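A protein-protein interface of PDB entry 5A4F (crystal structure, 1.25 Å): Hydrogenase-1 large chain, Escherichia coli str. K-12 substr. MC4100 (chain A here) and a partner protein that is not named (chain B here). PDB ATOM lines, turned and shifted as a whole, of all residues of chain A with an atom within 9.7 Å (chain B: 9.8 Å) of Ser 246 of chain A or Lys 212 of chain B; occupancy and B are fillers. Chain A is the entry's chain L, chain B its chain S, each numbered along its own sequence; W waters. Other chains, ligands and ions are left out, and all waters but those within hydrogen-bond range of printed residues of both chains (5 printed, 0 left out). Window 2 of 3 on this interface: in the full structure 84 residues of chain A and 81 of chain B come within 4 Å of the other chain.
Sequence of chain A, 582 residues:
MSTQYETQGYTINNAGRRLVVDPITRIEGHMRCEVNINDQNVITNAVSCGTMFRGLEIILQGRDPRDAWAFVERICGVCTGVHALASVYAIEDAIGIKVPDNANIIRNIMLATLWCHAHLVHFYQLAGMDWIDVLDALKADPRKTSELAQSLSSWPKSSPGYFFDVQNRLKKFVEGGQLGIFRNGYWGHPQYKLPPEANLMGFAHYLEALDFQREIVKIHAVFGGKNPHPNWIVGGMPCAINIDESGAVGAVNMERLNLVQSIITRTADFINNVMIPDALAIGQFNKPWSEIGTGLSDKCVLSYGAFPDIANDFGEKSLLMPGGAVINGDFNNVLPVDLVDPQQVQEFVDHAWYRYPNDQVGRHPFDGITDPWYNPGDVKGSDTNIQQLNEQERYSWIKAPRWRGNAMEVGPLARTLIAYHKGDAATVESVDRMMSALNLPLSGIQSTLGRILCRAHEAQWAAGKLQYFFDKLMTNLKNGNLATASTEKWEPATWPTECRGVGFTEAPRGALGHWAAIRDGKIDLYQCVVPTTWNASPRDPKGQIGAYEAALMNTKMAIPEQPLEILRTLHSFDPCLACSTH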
ATOM      1  N   PRO A 238       2.247  18.943  21.395  1.00  0.00           N
ATOM      2  CA  PRO A 238       3.074  20.021  21.984  1.00  0.00           C
ATOM      3  C   PRO A 238       4.108  19.521  22.994  1.00  0.00           C
ATOM      4  O   PRO A 238       4.927  20.347  23.453  1.00  0.00           O
ATOM      5  CB  PRO A 238       2.057  20.961  22.637  1.00  0.00           C
ATOM      6  CG  PRO A 238       0.797  20.263  22.722  1.00  0.00           C
ATOM      7  CD  PRO A 238       0.864  18.984  21.943  1.00  0.00           C
ATOM      8  N   CYS A 239       4.037  18.254  23.354  1.00  0.00           N
ATOM      9  CA  CYS A 239       4.856  17.676  24.391  1.00  0.00           C
ATOM     10  C   CYS A 239       6.248  17.294  23.867  1.00  0.00           C
ATOM     11  O   CYS A 239       6.558  16.093  23.688  1.00  0.00           O
ATOM     12  CB  CYS A 239       4.114  16.509  25.051  1.00  0.00           C
ATOM     13  SG  CYS A 239       3.539  15.262  23.858  1.00  0.00           S
ATOM     14  N   ALA A 240       7.089  18.307  23.705  1.00  0.00           N
ATOM     15  CA  ALA A 240       8.442  18.119  23.244  1.00  0.00           C
ATOM     16  C   ALA A 240       9.186  17.164  24.166  1.00  0.00           C
ATOM     17  O   ALA A 240       8.952  17.123  25.384  1.00  0.00           O
ATOM     18  CB  ALA A 240       9.134  19.467  23.221  1.00  0.00           C
ATOM     19  N   ILE A 241      10.048  16.364  23.544  1.00  0.00           N
ATOM     20  CA  ILE A 241      10.813  15.347  24.217  1.00  0.00           C
ATOM     21  C   ILE A 241      12.269  15.764  24.355  1.00  0.00           C
ATOM     22  O   ILE A 241      12.884  16.297  23.414  1.00  0.00           O
ATOM     23  CB  ILE A 241      10.718  14.021  23.427  1.00  0.00           C
ATOM     24  CG1 ILE A 241       9.260  13.532  23.343  1.00  0.00           C
ATOM     25  CG2 ILE A 241      11.600  12.914  24.055  1.00  0.00           C
ATOM     26  CD1 ILE A 241       9.045  12.353  22.424  1.00  0.00           C
ATOM     27  N   ASN A 242      12.849  15.452  25.514  1.00  0.00           N
ATOM     28  CA  ASN A 242      14.271  15.677  25.788  1.00  0.00           C
ATOM     29  C   ASN A 242      14.663  14.648  26.824  1.00  0.00           C
ATOM     30  O   ASN A 242      14.183  14.702  27.957  1.00  0.00           O
ATOM     31  CB  ASN A 242      14.523  17.103  26.237  1.00  0.00           C
ATOM     32  CG  ASN A 242      15.983  17.386  26.550  1.00  0.00           C
ATOM     33  OD1 ASN A 242      16.842  16.486  26.602  1.00  0.00           O
ATOM     34  ND2 ASN A 242      16.258  18.645  26.837  1.00  0.00           N
ATOM     35  N   ILE A 243      15.462  13.683  26.399  1.00  0.00           N
ATOM     36  CA  ILE A 243      15.905  12.612  27.264  1.00  0.00           C
ATOM     37  C   ILE A 243      17.265  12.857  27.881  1.00  0.00           C
ATOM     38  O   ILE A 243      17.451  12.522  29.048  1.00  0.00           O
ATOM     39  CB  ILE A 243      15.951  11.237  26.501  1.00  0.00           C
ATOM     40  CG1 ILE A 243      14.657  10.972  25.775  1.00  0.00           C
ATOM     41  CG2 ILE A 243      16.312  10.124  27.468  1.00  0.00           C
ATOM     42  CD1 ILE A 243      13.500  11.060  26.725  1.00  0.00           C
ATOM     43  N   ASP A 244      18.222  13.398  27.145  1.00  0.00           N
ATOM     44  CA  ASP A 244      19.646  13.350  27.588  1.00  0.00           C
ATOM     45  C   ASP A 244      20.382  14.650  27.414  1.00  0.00           C
ATOM     46  O   ASP A 244      21.617  14.656  27.379  1.00  0.00           O
ATOM     47  CB  ASP A 244      20.375  12.192  26.842  1.00  0.00           C
ATOM     48  CG  ASP A 244      21.746  11.889  27.368  1.00  0.00           C
ATOM     49  OD1 ASP A 244      21.953  11.822  28.602  1.00  0.00           O
ATOM     50  OD2 ASP A 244      22.661  11.616  26.544  1.00  0.00           O
ATOM     51  N   GLU A 245      19.655  15.778  27.328  1.00  0.00           N
ATOM     52  CA  GLU A 245      20.257  17.087  27.179  1.00  0.00           C
ATOM     53  C   GLU A 245      19.871  17.976  28.314  1.00  0.00           C
ATOM     54  O   GLU A 245      18.912  17.683  29.088  1.00  0.00           O
ATOM     55  CB  GLU A 245      19.853  17.698  25.823  1.00  0.00           C
ATOM     56  CG  GLU A 245      20.299  16.840  24.606  1.00  0.00           C
ATOM     57  CD  GLU A 245      19.408  17.117  23.407  1.00  0.00           C
ATOM     58  OE1 GLU A 245      19.707  18.155  22.877  1.00  0.00           O
ATOM     59  OE2 GLU A 245      18.403  16.362  23.050  1.00  0.00           O
ATOM     60  N   SER A 246      20.593  19.082  28.479  1.00  0.00           N
ATOM     61  CA  SER A 246      20.279  20.054  29.495  1.00  0.00           C
ATOM     62  C   SER A 246      18.850  20.531  29.297  1.00  0.00           C
ATOM     63  O   SER A 246      18.344  20.651  28.166  1.00  0.00           O
ATOM     64  CB  SER A 246      21.245  21.228  29.379  1.00  0.00           C
ATOM     65  OG  SER A 246      20.961  22.176  30.379  1.00  0.00           O
ATOM     66  N   GLY A 247      18.163  20.741  30.388  1.00  0.00           N
ATOM     67  CA  GLY A 247      16.793  21.217  30.279  1.00  0.00           C
ATOM     68  C   GLY A 247      15.747  20.132  30.041  1.00  0.00           C
ATOM     69  O   GLY A 247      14.577  20.446  29.819  1.00  0.00           O
ATOM     70  N   ALA A 248      16.130  18.862  30.212  1.00  0.00           N
ATOM     71  CA  ALA A 248      15.149  17.759  30.109  1.00  0.00           C
ATOM     72  C   ALA A 248      14.084  17.908  31.169  1.00  0.00           C
ATOM     73  O   ALA A 248      12.953  17.395  30.985  1.00  0.00           O
ATOM     74  CB  ALA A 248      15.820  16.404  30.204  1.00  0.00           C
ATOM     75  N   VAL A 249      14.386  18.616  32.265  1.00  0.00           N
ATOM     76  CA  VAL A 249      13.385  18.963  33.248  1.00  0.00           C
ATOM     77  C   VAL A 249      12.201  19.739  32.696  1.00  0.00           C
ATOM     78  O   VAL A 249      11.148  19.794  33.373  1.00  0.00           O
ATOM     79  CB  VAL A 249      14.004  19.698  34.463  1.00  0.00           C
ATOM     80  CG1 VAL A 249      14.936  18.785  35.262  1.00  0.00           C
ATOM     81  CG2 VAL A 249      14.642  20.988  34.111  1.00  0.00           C
ATOM     82  N   GLY A 250      12.412  20.396  31.556  1.00  0.00           N
ATOM     83  CA  GLY A 250      11.361  21.127  30.878  1.00  0.00           C
ATOM     84  C   GLY A 250      10.598  20.385  29.822  1.00  0.00           C
ATOM     85  O   GLY A 250       9.904  21.074  29.025  1.00  0.00           O
ATOM     86  N   ALA A 251      10.702  19.059  29.734  1.00  0.00           N
ATOM     87  CA  ALA A 251      10.187  18.304  28.609  1.00  0.00           C
ATOM     88  C   ALA A 251       9.770  16.904  29.034  1.00  0.00           C
ATOM     89  O   ALA A 251       9.927  16.511  30.198  1.00  0.00           O
ATOM     90  CB  ALA A 251      11.269  18.246  27.534  1.00  0.00           C
ATOM     91  N   VAL A 252       9.291  16.127  28.061  1.00  0.00           N
ATOM     92  CA  VAL A 252       9.045  14.720  28.306  1.00  0.00           C
ATOM     93  C   VAL A 252      10.402  14.047  28.400  1.00  0.00           C
ATOM     94  O   VAL A 252      11.125  13.917  27.400  1.00  0.00           O
ATOM     95  CB  VAL A 252       8.161  14.120  27.235  1.00  0.00           C
ATOM     96  CG1 VAL A 252       8.034  12.614  27.402  1.00  0.00           C
ATOM     97  CG2 VAL A 252       6.775  14.777  27.216  1.00  0.00           C
ATOM     98  N   ASN A 253      10.737  13.550  29.594  1.00  0.00           N
ATOM     99  CA  ASN A 253      12.058  12.994  29.902  1.00  0.00           C
ATOM    100  C   ASN A 253      11.880  11.555  30.388  1.00  0.00           C
ATOM    101  O   ASN A 253      10.774  11.016  30.387  1.00  0.00           O
ATOM    102  CB  ASN A 253      12.761  13.908  30.901  1.00  0.00           C
ATOM    103  CG  ASN A 253      11.996  14.038  32.186  1.00  0.00           C
ATOM    104  OD1 ASN A 253      11.519  13.055  32.730  1.00  0.00           O
ATOM    105  ND2 ASN A 253      11.870  15.225  32.677  1.00  0.00           N
ATOM    106  N   TYR B 191       6.162  27.905  36.797  1.00  0.00           N
ATOM    107  CA  TYR B 191       7.565  27.496  36.876  1.00  0.00           C
ATOM    108  C   TYR B 191       8.375  27.903  35.652  1.00  0.00           C
ATOM    109  O   TYR B 191       9.601  27.781  35.713  1.00  0.00           O
ATOM    110  CB  TYR B 191       7.651  25.964  37.158  1.00  0.00           C
ATOM    111  CG  TYR B 191       7.536  25.082  35.950  1.00  0.00           C
ATOM    112  CD1 TYR B 191       6.428  25.117  35.083  1.00  0.00           C
ATOM    113  CD2 TYR B 191       8.529  24.158  35.680  1.00  0.00           C
ATOM    114  CE1 TYR B 191       6.359  24.273  33.980  1.00  0.00           C
ATOM    115  CE2 TYR B 191       8.478  23.337  34.572  1.00  0.00           C
ATOM    116  CZ  TYR B 191       7.397  23.415  33.703  1.00  0.00           C
ATOM    117  OH  TYR B 191       7.323  22.656  32.542  1.00  0.00           O
ATOM    118  N   ARG B 192       7.767  28.388  34.564  1.00  0.00           N
ATOM    119  CA  ARG B 192       8.532  28.884  33.415  1.00  0.00           C
ATOM    120  C   ARG B 192       8.704  30.390  33.484  1.00  0.00           C
ATOM    121  O   ARG B 192       9.258  30.978  32.528  1.00  0.00           O
ATOM    122  CB  ARG B 192       7.885  28.456  32.078  1.00  0.00           C
ATOM    123  CG  ARG B 192       7.856  26.951  31.899  1.00  0.00           C
ATOM    124  CD  ARG B 192       7.346  26.523  30.566  1.00  0.00           C
ATOM    125  NE  ARG B 192       7.250  25.074  30.459  1.00  0.00           N
ATOM    126  CZ  ARG B 192       7.297  24.348  29.355  1.00  0.00           C
ATOM    127  NH1 ARG B 192       7.454  24.906  28.170  1.00  0.00           N
ATOM    128  NH2 ARG B 192       7.169  22.999  29.432  1.00  0.00           N
ATOM    129  N   ALA B 194      10.825  32.231  35.013  1.00  0.00           N
ATOM    130  CA  ALA B 194      12.209  32.637  34.849  1.00  0.00           C
ATOM    131  C   ALA B 194      12.528  32.890  33.374  1.00  0.00           C
ATOM    132  O   ALA B 194      13.266  33.827  33.021  1.00  0.00           O
ATOM    133  CB  ALA B 194      13.143  31.565  35.330  1.00  0.00           C
ATOM    134  N   HIS B 195      11.991  32.020  32.511  1.00  0.00           N
ATOM    135  CA  HIS B 195      12.226  32.166  31.073  1.00  0.00           C
ATOM    136  C   HIS B 195      11.506  33.382  30.465  1.00  0.00           C
ATOM    137  O   HIS B 195      12.099  34.148  29.676  1.00  0.00           O
ATOM    138  CB  HIS B 195      11.834  30.904  30.335  1.00  0.00           C
ATOM    139  CG  HIS B 195      12.573  29.699  30.815  1.00  0.00           C
ATOM    140  ND1 HIS B 195      13.950  29.635  30.832  1.00  0.00           N
ATOM    141  CD2 HIS B 195      12.142  28.521  31.308  1.00  0.00           C
ATOM    142  CE1 HIS B 195      14.332  28.455  31.304  1.00  0.00           C
ATOM    143  NE2 HIS B 195      13.246  27.757  31.585  1.00  0.00           N
ATOM    144  N   GLU B 200      13.209  34.273  27.088  1.00  0.00           N
ATOM    145  CA  GLU B 200      13.537  32.944  26.607  1.00  0.00           C
ATOM    146  C   GLU B 200      12.213  32.265  26.254  1.00  0.00           C
ATOM    147  O   GLU B 200      11.511  31.741  27.123  1.00  0.00           O
ATOM    148  CB  GLU B 200      14.290  32.171  27.694  1.00  0.00           C
ATOM    149  CG  GLU B 200      15.733  32.653  27.815  1.00  0.00           C
ATOM    150  CD  GLU B 200      16.490  32.096  28.987  1.00  0.00           C
ATOM    151  OE1 GLU B 200      15.908  31.477  29.886  1.00  0.00           O
ATOM    152  OE2 GLU B 200      17.713  32.342  29.043  1.00  0.00           O
ATOM    153  N   PHE B 201      11.907  32.222  24.969  1.00  0.00           N
ATOM    154  CA  PHE B 201      10.576  31.839  24.485  1.00  0.00           C
ATOM    155  C   PHE B 201      10.677  30.735  23.448  1.00  0.00           C
ATOM    156  O   PHE B 201      11.548  30.730  22.558  1.00  0.00           O
ATOM    157  CB  PHE B 201       9.908  33.016  23.818  1.00  0.00           C
ATOM    158  CG  PHE B 201       9.660  34.191  24.733  1.00  0.00           C
ATOM    159  CD1 PHE B 201       8.780  34.082  25.786  1.00  0.00           C
ATOM    160  CD2 PHE B 201      10.324  35.433  24.551  1.00  0.00           C
ATOM    161  CE1 PHE B 201       8.559  35.120  26.642  1.00  0.00           C
ATOM    162  CE2 PHE B 201      10.053  36.466  25.383  1.00  0.00           C
ATOM    163  CZ  PHE B 201       9.181  36.350  26.431  1.00  0.00           C
ATOM    164  N   VAL B 202       9.709  29.798  23.477  1.00  0.00           N
ATOM    165  CA  VAL B 202       9.405  28.913  22.356  1.00  0.00           C
ATOM    166  C   VAL B 202       8.890  29.795  21.210  1.00  0.00           C
ATOM    167  O   VAL B 202       8.026  30.652  21.401  1.00  0.00           O
ATOM    168  CB  VAL B 202       8.320  27.901  22.754  1.00  0.00           C
ATOM    169  CG1 VAL B 202       7.929  27.034  21.571  1.00  0.00           C
ATOM    170  CG2 VAL B 202       8.789  27.051  23.921  1.00  0.00           C
ATOM    171  N   SER B 204       8.585  28.246  17.788  1.00  0.00           N
ATOM    172  CA  SER B 204       7.841  27.312  16.991  1.00  0.00           C
ATOM    173  C   SER B 204       7.834  25.951  17.688  1.00  0.00           C
ATOM    174  O   SER B 204       8.744  25.642  18.456  1.00  0.00           O
ATOM    175  CB  SER B 204       8.364  27.209  15.567  1.00  0.00           C
ATOM    176  OG  SER B 204       9.648  26.755  15.532  1.00  0.00           O
ATOM    177  N   ASP B 206       8.393  22.390  19.071  1.00  0.00           N
ATOM    178  CA  ASP B 206       9.477  21.404  19.069  1.00  0.00           C
ATOM    179  C   ASP B 206      10.807  22.022  18.670  1.00  0.00           C
ATOM    180  O   ASP B 206      11.685  21.292  18.247  1.00  0.00           O
ATOM    181  CB  ASP B 206       9.112  20.189  18.238  1.00  0.00           C
ATOM    182  CG  ASP B 206       9.915  18.974  18.574  1.00  0.00           C
ATOM    183  OD1 ASP B 206      10.412  18.890  19.727  1.00  0.00           O
ATOM    184  OD2 ASP B 206      10.055  18.080  17.690  1.00  0.00           O
ATOM    185  N   ASP B 207      10.947  23.326  18.826  1.00  0.00           N
ATOM    186  CA  ASP B 207      12.233  23.988  18.642  1.00  0.00           C
ATOM    187  C   ASP B 207      13.131  23.731  19.871  1.00  0.00           C
ATOM    188  O   ASP B 207      12.734  23.057  20.828  1.00  0.00           O
ATOM    189  CB  ASP B 207      12.087  25.472  18.260  1.00  0.00           C
ATOM    190  CG  ASP B 207      11.525  26.377  19.347  1.00  0.00           C
ATOM    191  OD1 ASP B 207      11.270  25.954  20.488  1.00  0.00           O
ATOM    192  OD2 ASP B 207      11.349  27.599  19.055  1.00  0.00           O
ATOM    193  N   ASP B 208      14.372  24.199  19.843  1.00  0.00           N
ATOM    194  CA  ASP B 208      15.269  23.903  20.929  1.00  0.00           C
ATOM    195  C   ASP B 208      14.750  24.477  22.221  1.00  0.00           C
ATOM    196  O   ASP B 208      14.902  23.847  23.306  1.00  0.00           O
ATOM    197  CB  ASP B 208      16.674  24.403  20.570  1.00  0.00           C
ATOM    198  CG  ASP B 208      17.364  23.495  19.515  1.00  0.00           C
ATOM    199  OD1 ASP B 208      16.856  22.401  19.109  1.00  0.00           O
ATOM    200  OD2 ASP B 208      18.498  23.848  19.166  1.00  0.00           O
ATOM    201  N   ALA B 209      14.159  25.649  22.150  1.00  0.00           N
ATOM    202  CA  ALA B 209      13.534  26.258  23.324  1.00  0.00           C
ATOM    203  C   ALA B 209      12.444  25.385  23.949  1.00  0.00           C
ATOM    204  O   ALA B 209      12.358  25.238  25.177  1.00  0.00           O
ATOM    205  CB  ALA B 209      12.983  27.613  22.941  1.00  0.00           C
ATOM    206  N   ALA B 210      11.596  24.832  23.086  1.00  0.00           N
ATOM    207  CA  ALA B 210      10.537  23.951  23.588  1.00  0.00           C
ATOM    208  C   ALA B 210      11.096  22.749  24.331  1.00  0.00           C
ATOM    209  O   ALA B 210      10.558  22.284  25.309  1.00  0.00           O
ATOM    210  CB  ALA B 210       9.658  23.482  22.429  1.00  0.00           C
ATOM    211  N   ARG B 211      12.174  22.191  23.793  1.00  0.00           N
ATOM    212  CA  ARG B 211      12.832  21.062  24.401  1.00  0.00           C
ATOM    213  C   ARG B 211      13.575  21.362  25.701  1.00  0.00           C
ATOM    214  O   ARG B 211      13.965  20.376  26.394  1.00  0.00           O
ATOM    215  CB  ARG B 211      13.760  20.402  23.390  1.00  0.00           C
ATOM    216  CG  ARG B 211      13.021  19.763  22.211  1.00  0.00           C
ATOM    217  CD  ARG B 211      13.974  19.266  21.155  1.00  0.00           C
ATOM    218  NE  ARG B 211      13.215  18.705  20.037  1.00  0.00           N
ATOM    219  CZ  ARG B 211      13.715  17.854  19.128  1.00  0.00           C
ATOM    220  NH1 ARG B 211      14.994  17.466  19.144  1.00  0.00           N
ATOM    221  NH2 ARG B 211      12.926  17.357  18.182  1.00  0.00           N
ATOM    222  N   LYS B 212      13.690  22.640  26.055  1.00  0.00           N
ATOM    223  CA  LYS B 212      14.254  23.044  27.347  1.00  0.00           C
ATOM    224  C   LYS B 212      13.198  23.632  28.301  1.00  0.00           C
ATOM    225  O   LYS B 212      13.527  24.113  29.372  1.00  0.00           O
ATOM    226  CB  LYS B 212      15.336  24.108  27.103  1.00  0.00           C
ATOM    227  CG  LYS B 212      16.550  23.615  26.338  1.00  0.00           C
ATOM    228  CD  LYS B 212      17.508  24.804  26.240  1.00  0.00           C
ATOM    229  CE  LYS B 212      17.244  25.744  25.089  1.00  0.00           C
ATOM    230  NZ  LYS B 212      18.528  26.476  24.787  1.00  0.00           N
ATOM    231  N   GLY B 213      11.919  23.592  27.876  1.00  0.00           N
ATOM    232  CA  GLY B 213      10.863  24.105  28.719  1.00  0.00           C
ATOM    233  C   GLY B 213      10.791  25.611  28.827  1.00  0.00           C
ATOM    234  O   GLY B 213      10.408  26.138  29.858  1.00  0.00           O
ATOM    235  N   TYR B 214      11.132  26.350  27.750  1.00  0.00           N
ATOM    236  CA  TYR B 214      11.030  27.793  27.769  1.00  0.00           C
ATOM    237  C   TYR B 214       9.575  28.255  27.745  1.00  0.00           C
ATOM    238  O   TYR B 214       8.623  27.486  27.604  1.00  0.00           O
ATOM    239  CB  TYR B 214      11.842  28.381  26.593  1.00  0.00           C
ATOM    240  CG  TYR B 214      13.360  28.437  26.801  1.00  0.00           C
ATOM    241  CD1 TYR B 214      14.021  27.806  27.839  1.00  0.00           C
ATOM    242  CD2 TYR B 214      14.131  29.108  25.839  1.00  0.00           C
ATOM    243  CE1 TYR B 214      15.416  27.885  27.983  1.00  0.00           C
ATOM    244  CE2 TYR B 214      15.498  29.153  25.955  1.00  0.00           C
ATOM    245  CZ  TYR B 214      16.133  28.517  27.003  1.00  0.00           C
ATOM    246  OH  TYR B 214      17.523  28.588  27.137  1.00  0.00           O
ATOM    247  N   CYS B 215       9.402  29.537  28.013  1.00  0.00           N
ATOM    248  CA  CYS B 215       8.088  30.155  28.184  1.00  0.00           C
ATOM    249  C   CYS B 215       7.290  30.129  26.868  1.00  0.00           C
ATOM    250  O   CYS B 215       7.886  30.200  25.761  1.00  0.00           O
ATOM    251  CB  CYS B 215       8.264  31.579  28.733  1.00  0.00           C
ATOM    252  SG  CYS B 215       6.757  32.609  28.692  1.00  0.00           S
ATOM    253  N   LEU B 216       6.004  29.914  27.029  1.00  0.00           N
ATOM    254  CA  LEU B 216       5.012  29.777  25.953  1.00  0.00           C
ATOM    255  C   LEU B 216       4.269  31.048  25.585  1.00  0.00           C
ATOM    256  O   LEU B 216       3.310  30.997  24.771  1.00  0.00           O
ATOM    257  CB  LEU B 216       4.051  28.630  26.284  1.00  0.00           C
ATOM    258  CG  LEU B 216       4.777  27.335  26.489  1.00  0.00           C
ATOM    259  CD1 LEU B 216       3.877  26.256  27.079  1.00  0.00           C
ATOM    260  CD2 LEU B 216       5.322  26.751  25.209  1.00  0.00           C
ATOM    261  N   ILE B 243       0.782  23.964  30.538  1.00  0.00           N
ATOM    262  CA  ILE B 243       2.087  24.557  30.249  1.00  0.00           C
ATOM    263  C   ILE B 243       3.211  23.569  30.484  1.00  0.00           C
ATOM    264  O   ILE B 243       4.141  23.516  29.676  1.00  0.00           O
ATOM    265  CB  ILE B 243       2.239  25.830  31.072  1.00  0.00           C
ATOM    266  CG1 ILE B 243       1.354  26.933  30.565  1.00  0.00           C
ATOM    267  CG2 ILE B 243       3.681  26.301  31.192  1.00  0.00           C
ATOM    268  CD1 ILE B 243       0.832  27.877  31.623  1.00  0.00           C
ATOM    269  N   GLN B 244       3.134  22.728  31.530  1.00  0.00           N
ATOM    270  CA  GLN B 244       4.176  21.778  31.812  1.00  0.00           C
ATOM    271  C   GLN B 244       4.329  20.784  30.649  1.00  0.00           C
ATOM    272  O   GLN B 244       5.438  20.349  30.373  1.00  0.00           O
ATOM    273  CB  GLN B 244       3.899  21.049  33.109  1.00  0.00           C
ATOM    274  CG  GLN B 244       4.964  20.112  33.565  1.00  0.00           C
ATOM    275  CD  GLN B 244       4.603  19.562  34.950  1.00  0.00           C
ATOM    276  OE1 GLN B 244       4.287  20.341  35.892  1.00  0.00           O
ATOM    277  NE2 GLN B 244       4.774  18.352  35.106  1.00  0.00           N
ATOM    278  N   GLY B 246       3.660  21.519  27.524  1.00  0.00           N
ATOM    279  CA  GLY B 246       4.108  22.220  26.337  1.00  0.00           C
ATOM    280  C   GLY B 246       3.121  23.054  25.570  1.00  0.00           C
ATOM    281  O   GLY B 246       3.486  23.586  24.533  1.00  0.00           O
HETATM  282  O   HOH W   1      10.162  16.396  20.664  1.00  0.00           O
HETATM  283  O   HOH W   2       7.638  21.023  27.406  1.00  0.00           O
HETATM  284  O   HOH W   3       8.532  20.356  32.865  1.00  0.00           O
HETATM  285  O   HOH W   4       6.754  22.032  21.281  1.00  0.00           O
HETATM  286  O   HOH W   5       6.029  23.111  23.669  1.00  0.00           O
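O of Gly 247 of chain A sits close to O of Arg 211 of chain B (3.5 Å). The side-chain amide nitrogen (ND2) of Asn 242 of chain A sits at hydrogen-bond distance from the backbone carbonyl oxygen (O) of Arg 211 of chain B (2.9 Å). The backbone carbonyl oxygen (O) of Gly 250 of chain A sits at hydrogen-bond distance from the guanidinium group (NH2) of Arg 192 of chain B, 3.4 Å away. The backbone carbonyl oxygen (O) of Gly 250 of chain A lies close to the backbone NH (N) of Gly 213 of chain B.
ND2 of Asn 242 of chain A lies close to N of Ala 248 of chain A, at 3.4 Å. NH1 of Arg 192 of chain B lies within hydrogen-bond range of O of Tyr 214 of chain B (2.9 Å). OD1 of Asn 242 of chain A is in hydrogen-bond range of N of Asp 244 of chain A, 3.4 Å away. NH2 of Arg 192 of chain B lies within hydrogen-bond range of O of Gln 244 of chain B. NZ of Lys 212 of chain B sits at hydrogen-bond distance from OH of Tyr 214 of chain B (3.3 Å). The side-chain amide nitrogen of Asn 253 of chain A sits at hydrogen-bond distance from the backbone carbonyl oxygen of Ala 251 of chain A (3.4 Å).
O of Pro 238 of chain A touches CA of Gly 246 of chain B (3.5 Å). CB of Ala 240 of chain A touches OD1 of Asp 206 of chain B, at 3.8 Å. Ala 210 of chain B touches Ala 240 of chain A. Arg 211 of chain B touches Ile 241 of chain A. O of Ser 246 of chain A touches CG of Lys 212 of chain B (3.9 Å). Lys 212 of chain B touches Gly 247 of chain A (CA to O, 3.6 Å). Gly 250 of chain A touches Ala 210 of chain B. Gly 250 of chain A touches Lys 212 of chain B. Ala 251 of chain A touches Arg 211 of chain B (CB to O, 3.6 Å).
Ser 246 of chain A touches just one residue of chain B: Lys 212 (3.9 Å). Printed residues of chain A within 4 Å of Lys 212 of chain B: Ser 246 (3.9 Å), Gly 247 (3.6 Å) and Gly 250 (3.98 Å). Gly 247 of chain A touches just these residues of chain B: Arg 211 (3.5 Å) and Lys 212 (3.6 Å). Printed residues of chain B within 4 Å of Ala 251 of chain A: Arg 211 (3.6 Å). Of the printed residues of chain B, Ile 241 of chain A touches Arg 211. Printed residues of chain A within 4 Å of Gly 246 of chain B: Pro 238 (3.5 Å). Of the printed residues of chain A, Arg 192 of chain B touches Gly 250. The nearest residue of chain B that does not touch Ser 246 of chain A is Arg 211 of chain B (4.7 Å). The nearest printed residue of chain A that does not touch Lys 212 of chain B is Asn 242 of chain A (4.8 Å).
Printed residues of chain A that touch a printed residue of chain B: Pro 238, Ala 240, Ile 241, Asn 242, Ser 246, Gly 247, Gly 250 and Ala 251. Hydrophobic or aromatic side chains of chain A that line the printed part of chain B: Pro 238, Ala 240 and Ala 251. Of the 22 printed residues of chain B, 7 touch a printed residue of chain A. Among the printed residues, 13 pairs touch across the chains. Among the printed residues, no Asp or Glu carboxylate lies within 4 Å of a Lys or Arg side-chain nitrogen of the other chain.
Water W3 bridges the side-chain hydroxyl of Tyr 191 of chain B (2.6 Å) and the backbone carbonyl oxygen of Val 249 of chain A (2.7 Å). Water W1 bridges the side-chain carboxylate of Asp 206 of chain B (2.7 Å) and the backbone NH of Ile 241 of chain A (2.9 Å). Water W4 bridges the backbone NH of Asp 206 of chain B (2.8 Å) and the backbone carbonyl oxygen of Pro 238 of chain A (3.3 Å). Water W2 bridges the backbone carbonyl oxygen of Gly 250 of chain A (2.8 Å) and the guanidinium group of Arg 192 of chain B (2.9 Å).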
